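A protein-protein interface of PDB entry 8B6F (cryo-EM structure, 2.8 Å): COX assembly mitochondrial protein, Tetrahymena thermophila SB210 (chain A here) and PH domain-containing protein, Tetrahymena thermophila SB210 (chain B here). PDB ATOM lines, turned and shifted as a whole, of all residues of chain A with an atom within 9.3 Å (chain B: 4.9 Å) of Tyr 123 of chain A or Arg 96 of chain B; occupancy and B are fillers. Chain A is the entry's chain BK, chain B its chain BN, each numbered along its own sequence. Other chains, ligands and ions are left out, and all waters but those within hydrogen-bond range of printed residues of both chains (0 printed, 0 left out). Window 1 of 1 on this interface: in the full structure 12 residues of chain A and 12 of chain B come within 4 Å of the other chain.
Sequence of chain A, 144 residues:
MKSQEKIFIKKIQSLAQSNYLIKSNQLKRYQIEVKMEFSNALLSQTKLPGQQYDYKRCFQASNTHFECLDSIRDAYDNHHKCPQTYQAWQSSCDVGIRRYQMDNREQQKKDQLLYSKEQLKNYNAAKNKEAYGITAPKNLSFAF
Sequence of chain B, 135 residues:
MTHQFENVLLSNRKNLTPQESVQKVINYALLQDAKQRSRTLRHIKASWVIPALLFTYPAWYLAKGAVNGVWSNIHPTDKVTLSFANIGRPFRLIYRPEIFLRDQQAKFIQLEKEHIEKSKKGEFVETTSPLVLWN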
ATOM      1  N   TYR A 115     -18.437 -21.283  11.199  1.00  0.00           N
ATOM      2  CA  TYR A 115     -19.891 -21.349  11.226  1.00  0.00           C
ATOM      3  C   TYR A 115     -20.480 -21.056   9.850  1.00  0.00           C
ATOM      4  O   TYR A 115     -19.774 -20.749   8.886  1.00  0.00           O
ATOM      5  CB  TYR A 115     -20.445 -20.368  12.261  1.00  0.00           C
ATOM      6  CG  TYR A 115     -19.689 -20.383  13.563  1.00  0.00           C
ATOM      7  CD1 TYR A 115     -19.967 -21.330  14.536  1.00  0.00           C
ATOM      8  CD2 TYR A 115     -18.691 -19.455  13.815  1.00  0.00           C
ATOM      9  CE1 TYR A 115     -19.275 -21.351  15.723  1.00  0.00           C
ATOM     10  CE2 TYR A 115     -17.993 -19.468  15.001  1.00  0.00           C
ATOM     11  CZ  TYR A 115     -18.292 -20.418  15.950  1.00  0.00           C
ATOM     12  OH  TYR A 115     -17.602 -20.437  17.134  1.00  0.00           O
ATOM     13  N   SER A 116     -21.805 -21.161   9.777  1.00  0.00           N
ATOM     14  CA  SER A 116     -22.568 -20.833   8.585  1.00  0.00           C
ATOM     15  C   SER A 116     -23.856 -20.140   9.006  1.00  0.00           C
ATOM     16  O   SER A 116     -24.286 -20.235  10.158  1.00  0.00           O
ATOM     17  CB  SER A 116     -22.884 -22.079   7.746  1.00  0.00           C
ATOM     18  OG  SER A 116     -23.756 -22.955   8.437  1.00  0.00           O
ATOM     19  N   LYS A 117     -24.472 -19.436   8.057  1.00  0.00           N
ATOM     20  CA  LYS A 117     -25.661 -18.650   8.372  1.00  0.00           C
ATOM     21  C   LYS A 117     -26.792 -19.540   8.875  1.00  0.00           C
ATOM     22  O   LYS A 117     -27.372 -19.285   9.936  1.00  0.00           O
ATOM     23  CB  LYS A 117     -26.100 -17.857   7.142  1.00  0.00           C
ATOM     24  CG  LYS A 117     -27.375 -17.055   7.347  1.00  0.00           C
ATOM     25  CD  LYS A 117     -27.635 -16.102   6.188  1.00  0.00           C
ATOM     26  CE  LYS A 117     -27.827 -16.837   4.868  1.00  0.00           C
ATOM     27  NZ  LYS A 117     -28.946 -17.820   4.922  1.00  0.00           N
ATOM     28  N   GLU A 118     -27.125 -20.587   8.120  1.00  0.00           N
ATOM     29  CA  GLU A 118     -28.222 -21.466   8.515  1.00  0.00           C
ATOM     30  C   GLU A 118     -27.903 -22.201   9.811  1.00  0.00           C
ATOM     31  O   GLU A 118     -28.777 -22.366  10.669  1.00  0.00           O
ATOM     32  CB  GLU A 118     -28.525 -22.460   7.395  1.00  0.00           C
ATOM     33  CG  GLU A 118     -29.736 -23.347   7.655  1.00  0.00           C
ATOM     34  CD  GLU A 118     -31.041 -22.569   7.695  1.00  0.00           C
ATOM     35  OE1 GLU A 118     -31.025 -21.358   7.392  1.00  0.00           O
ATOM     36  OE2 GLU A 118     -32.083 -23.172   8.029  1.00  0.00           O
ATOM     37  N   GLN A 119     -26.660 -22.659   9.967  1.00  0.00           N
ATOM     38  CA  GLN A 119     -26.267 -23.347  11.191  1.00  0.00           C
ATOM     39  C   GLN A 119     -26.441 -22.443  12.403  1.00  0.00           C
ATOM     40  O   GLN A 119     -26.990 -22.856  13.430  1.00  0.00           O
ATOM     41  CB  GLN A 119     -24.817 -23.820  11.072  1.00  0.00           C
ATOM     42  CG  GLN A 119     -24.273 -24.522  12.307  1.00  0.00           C
ATOM     43  CD  GLN A 119     -22.791 -24.807  12.197  1.00  0.00           C
ATOM     44  OE1 GLN A 119     -22.132 -24.375  11.253  1.00  0.00           O
ATOM     45  NE2 GLN A 119     -22.256 -25.542  13.164  1.00  0.00           N
ATOM     46  N   LEU A 120     -25.973 -21.197  12.302  1.00  0.00           N
ATOM     47  CA  LEU A 120     -26.112 -20.264  13.414  1.00  0.00           C
ATOM     48  C   LEU A 120     -27.576 -19.956  13.693  1.00  0.00           C
ATOM     49  O   LEU A 120     -27.984 -19.853  14.856  1.00  0.00           O
ATOM     50  CB  LEU A 120     -25.340 -18.979  13.118  1.00  0.00           C
ATOM     51  CG  LEU A 120     -23.814 -19.103  13.095  1.00  0.00           C
ATOM     52  CD1 LEU A 120     -23.185 -17.789  12.668  1.00  0.00           C
ATOM     53  CD2 LEU A 120     -23.275 -19.536  14.450  1.00  0.00           C
ATOM     54  N   LYS A 121     -28.384 -19.799  12.645  1.00  0.00           N
ATOM     55  CA  LYS A 121     -29.804 -19.538  12.848  1.00  0.00           C
ATOM     56  C   LYS A 121     -30.458 -20.673  13.625  1.00  0.00           C
ATOM     57  O   LYS A 121     -31.170 -20.440  14.607  1.00  0.00           O
ATOM     58  CB  LYS A 121     -30.494 -19.335  11.499  1.00  0.00           C
ATOM     59  CG  LYS A 121     -31.950 -18.912  11.606  1.00  0.00           C
ATOM     60  CD  LYS A 121     -32.560 -18.684  10.232  1.00  0.00           C
ATOM     61  CE  LYS A 121     -33.992 -18.183  10.336  1.00  0.00           C
ATOM     62  NZ  LYS A 121     -34.880 -19.151  11.034  1.00  0.00           N
ATOM     63  N   ASN A 122     -30.225 -21.914  13.195  1.00  0.00           N
ATOM     64  CA  ASN A 122     -30.823 -23.055  13.880  1.00  0.00           C
ATOM     65  C   ASN A 122     -30.324 -23.164  15.315  1.00  0.00           C
ATOM     66  O   ASN A 122     -31.105 -23.431  16.234  1.00  0.00           O
ATOM     67  CB  ASN A 122     -30.517 -24.342  13.114  1.00  0.00           C
ATOM     68  CG  ASN A 122     -31.177 -24.380  11.754  1.00  0.00           C
ATOM     69  OD1 ASN A 122     -32.249 -23.812  11.556  1.00  0.00           O
ATOM     70  ND2 ASN A 122     -30.537 -25.052  10.805  1.00  0.00           N
ATOM     71  N   TYR A 123     -29.020 -22.968  15.525  1.00  0.00           N
ATOM     72  CA  TYR A 123     -28.464 -23.074  16.870  1.00  0.00           C
ATOM     73  C   TYR A 123     -29.043 -22.012  17.797  1.00  0.00           C
ATOM     74  O   TYR A 123     -29.406 -22.309  18.942  1.00  0.00           O
ATOM     75  CB  TYR A 123     -26.942 -22.959  16.811  1.00  0.00           C
ATOM     76  CG  TYR A 123     -26.304 -22.712  18.153  1.00  0.00           C
ATOM     77  CD1 TYR A 123     -26.126 -23.749  19.057  1.00  0.00           C
ATOM     78  CD2 TYR A 123     -25.869 -21.445  18.512  1.00  0.00           C
ATOM     79  CE1 TYR A 123     -25.542 -23.530  20.283  1.00  0.00           C
ATOM     80  CE2 TYR A 123     -25.283 -21.218  19.734  1.00  0.00           C
ATOM     81  CZ  TYR A 123     -25.121 -22.264  20.613  1.00  0.00           C
ATOM     82  OH  TYR A 123     -24.537 -22.036  21.832  1.00  0.00           O
ATOM     83  N   ASN A 124     -29.138 -20.770  17.324  1.00  0.00           N
ATOM     84  CA  ASN A 124     -29.697 -19.711  18.158  1.00  0.00           C
ATOM     85  C   ASN A 124     -31.164 -19.970  18.464  1.00  0.00           C
ATOM     86  O   ASN A 124     -31.622 -19.736  19.588  1.00  0.00           O
ATOM     87  CB  ASN A 124     -29.518 -18.355  17.477  1.00  0.00           C
ATOM     88  CG  ASN A 124     -28.061 -17.955  17.352  1.00  0.00           C
ATOM     89  OD1 ASN A 124     -27.570 -17.692  16.257  1.00  0.00           O
ATOM     90  ND2 ASN A 124     -27.364 -17.900  18.480  1.00  0.00           N
ATOM     91  N   ALA A 125     -31.922 -20.448  17.477  1.00  0.00           N
ATOM     92  CA  ALA A 125     -33.320 -20.778  17.727  1.00  0.00           C
ATOM     93  C   ALA A 125     -33.443 -21.869  18.781  1.00  0.00           C
ATOM     94  O   ALA A 125     -34.274 -21.774  19.690  1.00  0.00           O
ATOM     95  CB  ALA A 125     -33.997 -21.211  16.427  1.00  0.00           C
ATOM     96  N   ALA A 126     -32.625 -22.917  18.673  1.00  0.00           N
ATOM     97  CA  ALA A 126     -32.678 -23.996  19.651  1.00  0.00           C
ATOM     98  C   ALA A 126     -32.301 -23.498  21.039  1.00  0.00           C
ATOM     99  O   ALA A 126     -32.918 -23.887  22.038  1.00  0.00           O
ATOM    100  CB  ALA A 126     -31.755 -25.137  19.223  1.00  0.00           C
ATOM    101  N   LYS A 127     -31.278 -22.642  21.125  1.00  0.00           N
ATOM    102  CA  LYS A 127     -30.853 -22.129  22.422  1.00  0.00           C
ATOM    103  C   LYS A 127     -31.923 -21.242  23.045  1.00  0.00           C
ATOM    104  O   LYS A 127     -32.167 -21.311  24.254  1.00  0.00           O
ATOM    105  CB  LYS A 127     -29.539 -21.364  22.274  1.00  0.00           C
ATOM    106  CG  LYS A 127     -28.684 -21.370  23.527  1.00  0.00           C
ATOM    107  CD  LYS A 127     -28.005 -22.713  23.732  1.00  0.00           C
ATOM    108  CE  LYS A 127     -27.197 -22.726  25.018  1.00  0.00           C
ATOM    109  NZ  LYS A 127     -26.501 -24.026  25.226  1.00  0.00           N
ATOM    110  N   ASN A 128     -32.566 -20.393  22.240  1.00  0.00           N
ATOM    111  CA  ASN A 128     -33.642 -19.557  22.761  1.00  0.00           C
ATOM    112  C   ASN A 128     -34.817 -20.404  23.227  1.00  0.00           C
ATOM    113  O   ASN A 128     -35.449 -20.098  24.244  1.00  0.00           O
ATOM    114  CB  ASN A 128     -34.088 -18.552  21.700  1.00  0.00           C
ATOM    115  CG  ASN A 128     -33.015 -17.528  21.380  1.00  0.00           C
ATOM    116  OD1 ASN A 128     -32.193 -17.189  22.227  1.00  0.00           O
ATOM    117  ND2 ASN A 128     -33.022 -17.029  20.150  1.00  0.00           N
ATOM    118  N   LYS A 129     -35.132 -21.471  22.489  1.00  0.00           N
ATOM    119  CA  LYS A 129     -36.178 -22.391  22.925  1.00  0.00           C
ATOM    120  C   LYS A 129     -35.801 -23.062  24.238  1.00  0.00           C
ATOM    121  O   LYS A 129     -36.646 -23.229  25.125  1.00  0.00           O
ATOM    122  CB  LYS A 129     -36.436 -23.438  21.841  1.00  0.00           C
ATOM    123  CG  LYS A 129     -37.459 -24.497  22.228  1.00  0.00           C
ATOM    124  CD  LYS A 129     -37.709 -25.469  21.084  1.00  0.00           C
ATOM    125  CE  LYS A 129     -38.628 -26.602  21.511  1.00  0.00           C
ATOM    126  NZ  LYS A 129     -39.948 -26.105  21.991  1.00  0.00           N
ATOM    127  N   GLU A 130     -34.536 -23.460  24.377  1.00  0.00           N
ATOM    128  CA  GLU A 130     -34.085 -24.098  25.608  1.00  0.00           C
ATOM    129  C   GLU A 130     -34.148 -23.144  26.792  1.00  0.00           C
ATOM    130  O   GLU A 130     -34.404 -23.578  27.921  1.00  0.00           O
ATOM    131  CB  GLU A 130     -32.659 -24.620  25.434  1.00  0.00           C
ATOM    132  CG  GLU A 130     -32.086 -25.300  26.673  1.00  0.00           C
ATOM    133  CD  GLU A 130     -30.604 -25.590  26.548  1.00  0.00           C
ATOM    134  OE1 GLU A 130     -29.959 -25.019  25.644  1.00  0.00           O
ATOM    135  OE2 GLU A 130     -30.082 -26.388  27.354  1.00  0.00           O
ATOM    136  N   ALA A 131     -33.913 -21.852  26.562  1.00  0.00           N
ATOM    137  CA  ALA A 131     -33.844 -20.904  27.667  1.00  0.00           C
ATOM    138  C   ALA A 131     -35.127 -20.871  28.483  1.00  0.00           C
ATOM    139  O   ALA A 131     -35.096 -20.459  29.646  1.00  0.00           O
ATOM    140  CB  ALA A 131     -33.532 -19.507  27.134  1.00  0.00           C
ATOM    141  N   ARG B  92     -20.066 -14.817  27.037  1.00  0.00           N
ATOM    142  CA  ARG B  92     -20.044 -15.795  25.957  1.00  0.00           C
ATOM    143  C   ARG B  92     -20.036 -17.214  26.505  1.00  0.00           C
ATOM    144  O   ARG B  92     -20.609 -18.120  25.893  1.00  0.00           O
ATOM    145  CB  ARG B  92     -18.823 -15.573  25.068  1.00  0.00           C
ATOM    146  CG  ARG B  92     -18.962 -14.438  24.069  1.00  0.00           C
ATOM    147  CD  ARG B  92     -17.692 -14.292  23.250  1.00  0.00           C
ATOM    148  NE  ARG B  92     -17.366 -15.523  22.542  1.00  0.00           N
ATOM    149  CZ  ARG B  92     -16.201 -15.772  21.961  1.00  0.00           C
ATOM    150  NH1 ARG B  92     -15.212 -14.894  21.991  1.00  0.00           N
ATOM    151  NH2 ARG B  92     -16.023 -16.931  21.336  1.00  0.00           N
ATOM    152  N   ILE B  94     -21.294 -17.998  29.593  1.00  0.00           N
ATOM    153  CA  ILE B  94     -22.565 -18.183  30.287  1.00  0.00           C
ATOM    154  C   ILE B  94     -23.676 -18.471  29.285  1.00  0.00           C
ATOM    155  O   ILE B  94     -24.448 -19.424  29.444  1.00  0.00           O
ATOM    156  CB  ILE B  94     -22.888 -16.952  31.153  1.00  0.00           C
ATOM    157  CG1 ILE B  94     -21.737 -16.648  32.118  1.00  0.00           C
ATOM    158  CG2 ILE B  94     -24.175 -17.171  31.936  1.00  0.00           C
ATOM    159  CD1 ILE B  94     -21.307 -17.817  32.979  1.00  0.00           C
ATOM    160  N   TYR B  95     -23.770 -17.656  28.238  1.00  0.00           N
ATOM    161  CA  TYR B  95     -24.746 -17.831  27.174  1.00  0.00           C
ATOM    162  C   TYR B  95     -24.029 -18.279  25.910  1.00  0.00           C
ATOM    163  O   TYR B  95     -22.975 -17.741  25.562  1.00  0.00           O
ATOM    164  CB  TYR B  95     -25.507 -16.532  26.883  1.00  0.00           C
ATOM    165  CG  TYR B  95     -26.105 -15.855  28.092  1.00  0.00           C
ATOM    166  CD1 TYR B  95     -25.312 -15.142  28.980  1.00  0.00           C
ATOM    167  CD2 TYR B  95     -27.472 -15.890  28.320  1.00  0.00           C
ATOM    168  CE1 TYR B  95     -25.859 -14.509  30.077  1.00  0.00           C
ATOM    169  CE2 TYR B  95     -28.029 -15.262  29.413  1.00  0.00           C
ATOM    170  CZ  TYR B  95     -27.219 -14.573  30.289  1.00  0.00           C
ATOM    171  OH  TYR B  95     -27.774 -13.944  31.377  1.00  0.00           O
ATOM    172  N   ARG B  96     -24.608 -19.247  25.220  1.00  0.00           N
ATOM    173  CA  ARG B  96     -24.029 -19.742  23.978  1.00  0.00           C
ATOM    174  C   ARG B  96     -22.658 -20.363  24.223  1.00  0.00           C
ATOM    175  O   ARG B  96     -21.685 -19.983  23.562  1.00  0.00           O
ATOM    176  CB  ARG B  96     -23.902 -18.614  22.949  1.00  0.00           C
ATOM    177  CG  ARG B  96     -25.166 -17.795  22.745  1.00  0.00           C
ATOM    178  CD  ARG B  96     -26.256 -18.628  22.101  1.00  0.00           C
ATOM    179  NE  ARG B  96     -27.483 -17.867  21.894  1.00  0.00           N
ATOM    180  CZ  ARG B  96     -28.403 -17.658  22.825  1.00  0.00           C
ATOM    181  NH1 ARG B  96     -28.257 -18.113  24.058  1.00  0.00           N
ATOM    182  NH2 ARG B  96     -29.499 -16.976  22.510  1.00  0.00           N
ATOM    183  N   PRO B  97     -22.532 -21.314  25.152  1.00  0.00           N
ATOM    184  CA  PRO B  97     -21.218 -21.935  25.378  1.00  0.00           C
ATOM    185  C   PRO B  97     -20.686 -22.693  24.175  1.00  0.00           C
ATOM    186  O   PRO B  97     -19.467 -22.857  24.059  1.00  0.00           O
ATOM    187  CB  PRO B  97     -21.470 -22.871  26.568  1.00  0.00           C
ATOM    188  CG  PRO B  97     -22.927 -23.132  26.548  1.00  0.00           C
ATOM    189  CD  PRO B  97     -23.568 -21.882  26.032  1.00  0.00           C
ATOM    190  N   GLU B  98     -21.556 -23.164  23.279  1.00  0.00           N
ATOM    191  CA  GLU B  98     -21.085 -23.925  22.126  1.00  0.00           C
ATOM    192  C   GLU B  98     -20.220 -23.064  21.217  1.00  0.00           C
ATOM    193  O   GLU B  98     -19.163 -23.503  20.753  1.00  0.00           O
ATOM    194  CB  GLU B  98     -22.269 -24.494  21.346  1.00  0.00           C
ATOM    195  CG  GLU B  98     -23.053 -25.566  22.079  1.00  0.00           C
ATOM    196  CD  GLU B  98     -23.960 -25.003  23.154  1.00  0.00           C
ATOM    197  OE1 GLU B  98     -23.855 -23.796  23.453  1.00  0.00           O
ATOM    198  OE2 GLU B  98     -24.784 -25.765  23.700  1.00  0.00           O
ATOM    199  N   ILE B  99     -20.661 -21.836  20.941  1.00  0.00           N
ATOM    200  CA  ILE B  99     -19.879 -20.934  20.100  1.00  0.00           C
ATOM    201  C   ILE B  99     -18.564 -20.584  20.783  1.00  0.00           C
ATOM    202  O   ILE B  99     -17.515 -20.484  20.136  1.00  0.00           O
ATOM    203  CB  ILE B  99     -20.698 -19.675  19.762  1.00  0.00           C
ATOM    204  CG1 ILE B  99     -21.938 -20.060  18.950  1.00  0.00           C
ATOM    205  CG2 ILE B  99     -19.850 -18.671  18.989  1.00  0.00           C
ATOM    206  CD1 ILE B  99     -22.941 -18.941  18.795  1.00  0.00           C
ATOM    207  N   PHE B 100     -18.602 -20.385  22.101  1.00  0.00           N
ATOM    208  CA  PHE B 100     -17.381 -20.109  22.850  1.00  0.00           C
ATOM    209  C   PHE B 100     -16.375 -21.240  22.683  1.00  0.00           C
ATOM    210  O   PHE B 100     -15.195 -21.002  22.400  1.00  0.00           O
ATOM    211  CB  PHE B 100     -17.728 -19.896  24.325  1.00  0.00           C
ATOM    212  CG  PHE B 100     -16.547 -19.561  25.188  1.00  0.00           C
ATOM    213  CD1 PHE B 100     -16.074 -18.262  25.263  1.00  0.00           C
ATOM    214  CD2 PHE B 100     -15.929 -20.538  25.949  1.00  0.00           C
ATOM    215  CE1 PHE B 100     -14.995 -17.948  26.063  1.00  0.00           C
ATOM    216  CE2 PHE B 100     -14.850 -20.229  26.752  1.00  0.00           C
ATOM    217  CZ  PHE B 100     -14.383 -18.933  26.809  1.00  0.00           C
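The backbone carbonyl oxygen (O) of Ile 99 of chain B sits at hydrogen-bond distance from the side-chain hydroxyl (OH) of Tyr 115 of chain A (3.0 Å).
The side-chain hydroxyl of Tyr 123 of chain A lies within hydrogen-bond range of the side-chain carboxylate of Glu 98 of chain B, 2.5 Å away.
The guanidinium group of Arg 96 of chain B sits close to the side-chain amide nitrogen of Asn 124 of chain A (3.4 Å).
The side-chain amino group (NZ) of Lys 127 of chain A lies within salt-bridge range of the side-chain carboxylate (OE2) of Glu 98 of chain B, 2.9 Å away.
The side-chain amide oxygen of Asn 128 of chain A lies within hydrogen-bond range of the guanidinium group of Arg 96 of chain B (2.7 Å).
The backbone carbonyl oxygen of Leu 120 of chain A lies close to the side-chain amide oxygen of Asn 124 of chain A.
The backbone carbonyl oxygen of Asn 124 of chain A lies within hydrogen-bond range of the side-chain amide nitrogen of Asn 128 of chain A.
The side-chain carboxylate (OE1) of Glu 130 of chain A is in salt-bridge range of the side-chain amino group (NZ) of Lys 127 of chain A (3.6 Å).
Among the printed residues, pairs that only touch across the chains: Tyr 123 of chain A with Arg 96 of chain B (3.2 Å), Lys 127 of chain A with Arg 96 of chain B (3.3 Å), Tyr 123 of chain A with Ile 99 of chain B (3.4 Å), Lys 127 of chain A with Pro 97 of chain B (3.7 Å) and Tyr 123 of chain A with Pro 97 of chain B (3.9 Å).
Of the printed residues of chain B, Tyr 115 of chain A touches Ile 99.
Printed residues of chain B within 4 Å of Tyr 123 of chain A: Arg 96, Pro 97, Glu 98 and Ile 99.
Printed residues of chain B within 4 Å of Lys 127 of chain A: Arg 96 (3.3 Å), Pro 97 (3.7 Å) and Glu 98 (2.9 Å).
Of the printed residues of chain B, Asn 128 of chain A touches Arg 96.
Ile 94 of chain B touches none of the printed residues of chain A.
Of chain A, only Tyr 123 (3.9 Å) and Lys 127 (3.7 Å) come within 4 Å of Pro 97 of chain B.
Of the printed residues of chain A, Ile 99 of chain B touches Tyr 115 and Tyr 123.
The nearest printed residue of chain B that does not touch Lys 127 of chain A is Tyr 95 of chain B (5.5 Å).
Of the 8 printed residues of chain B, 4 touch a printed residue of chain A.
Printed residues of chain B that touch a printed residue of chain A: Arg 96, Pro 97, Glu 98 and Ile 99.
Among the printed residues, 10 pairs touch across the chains.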
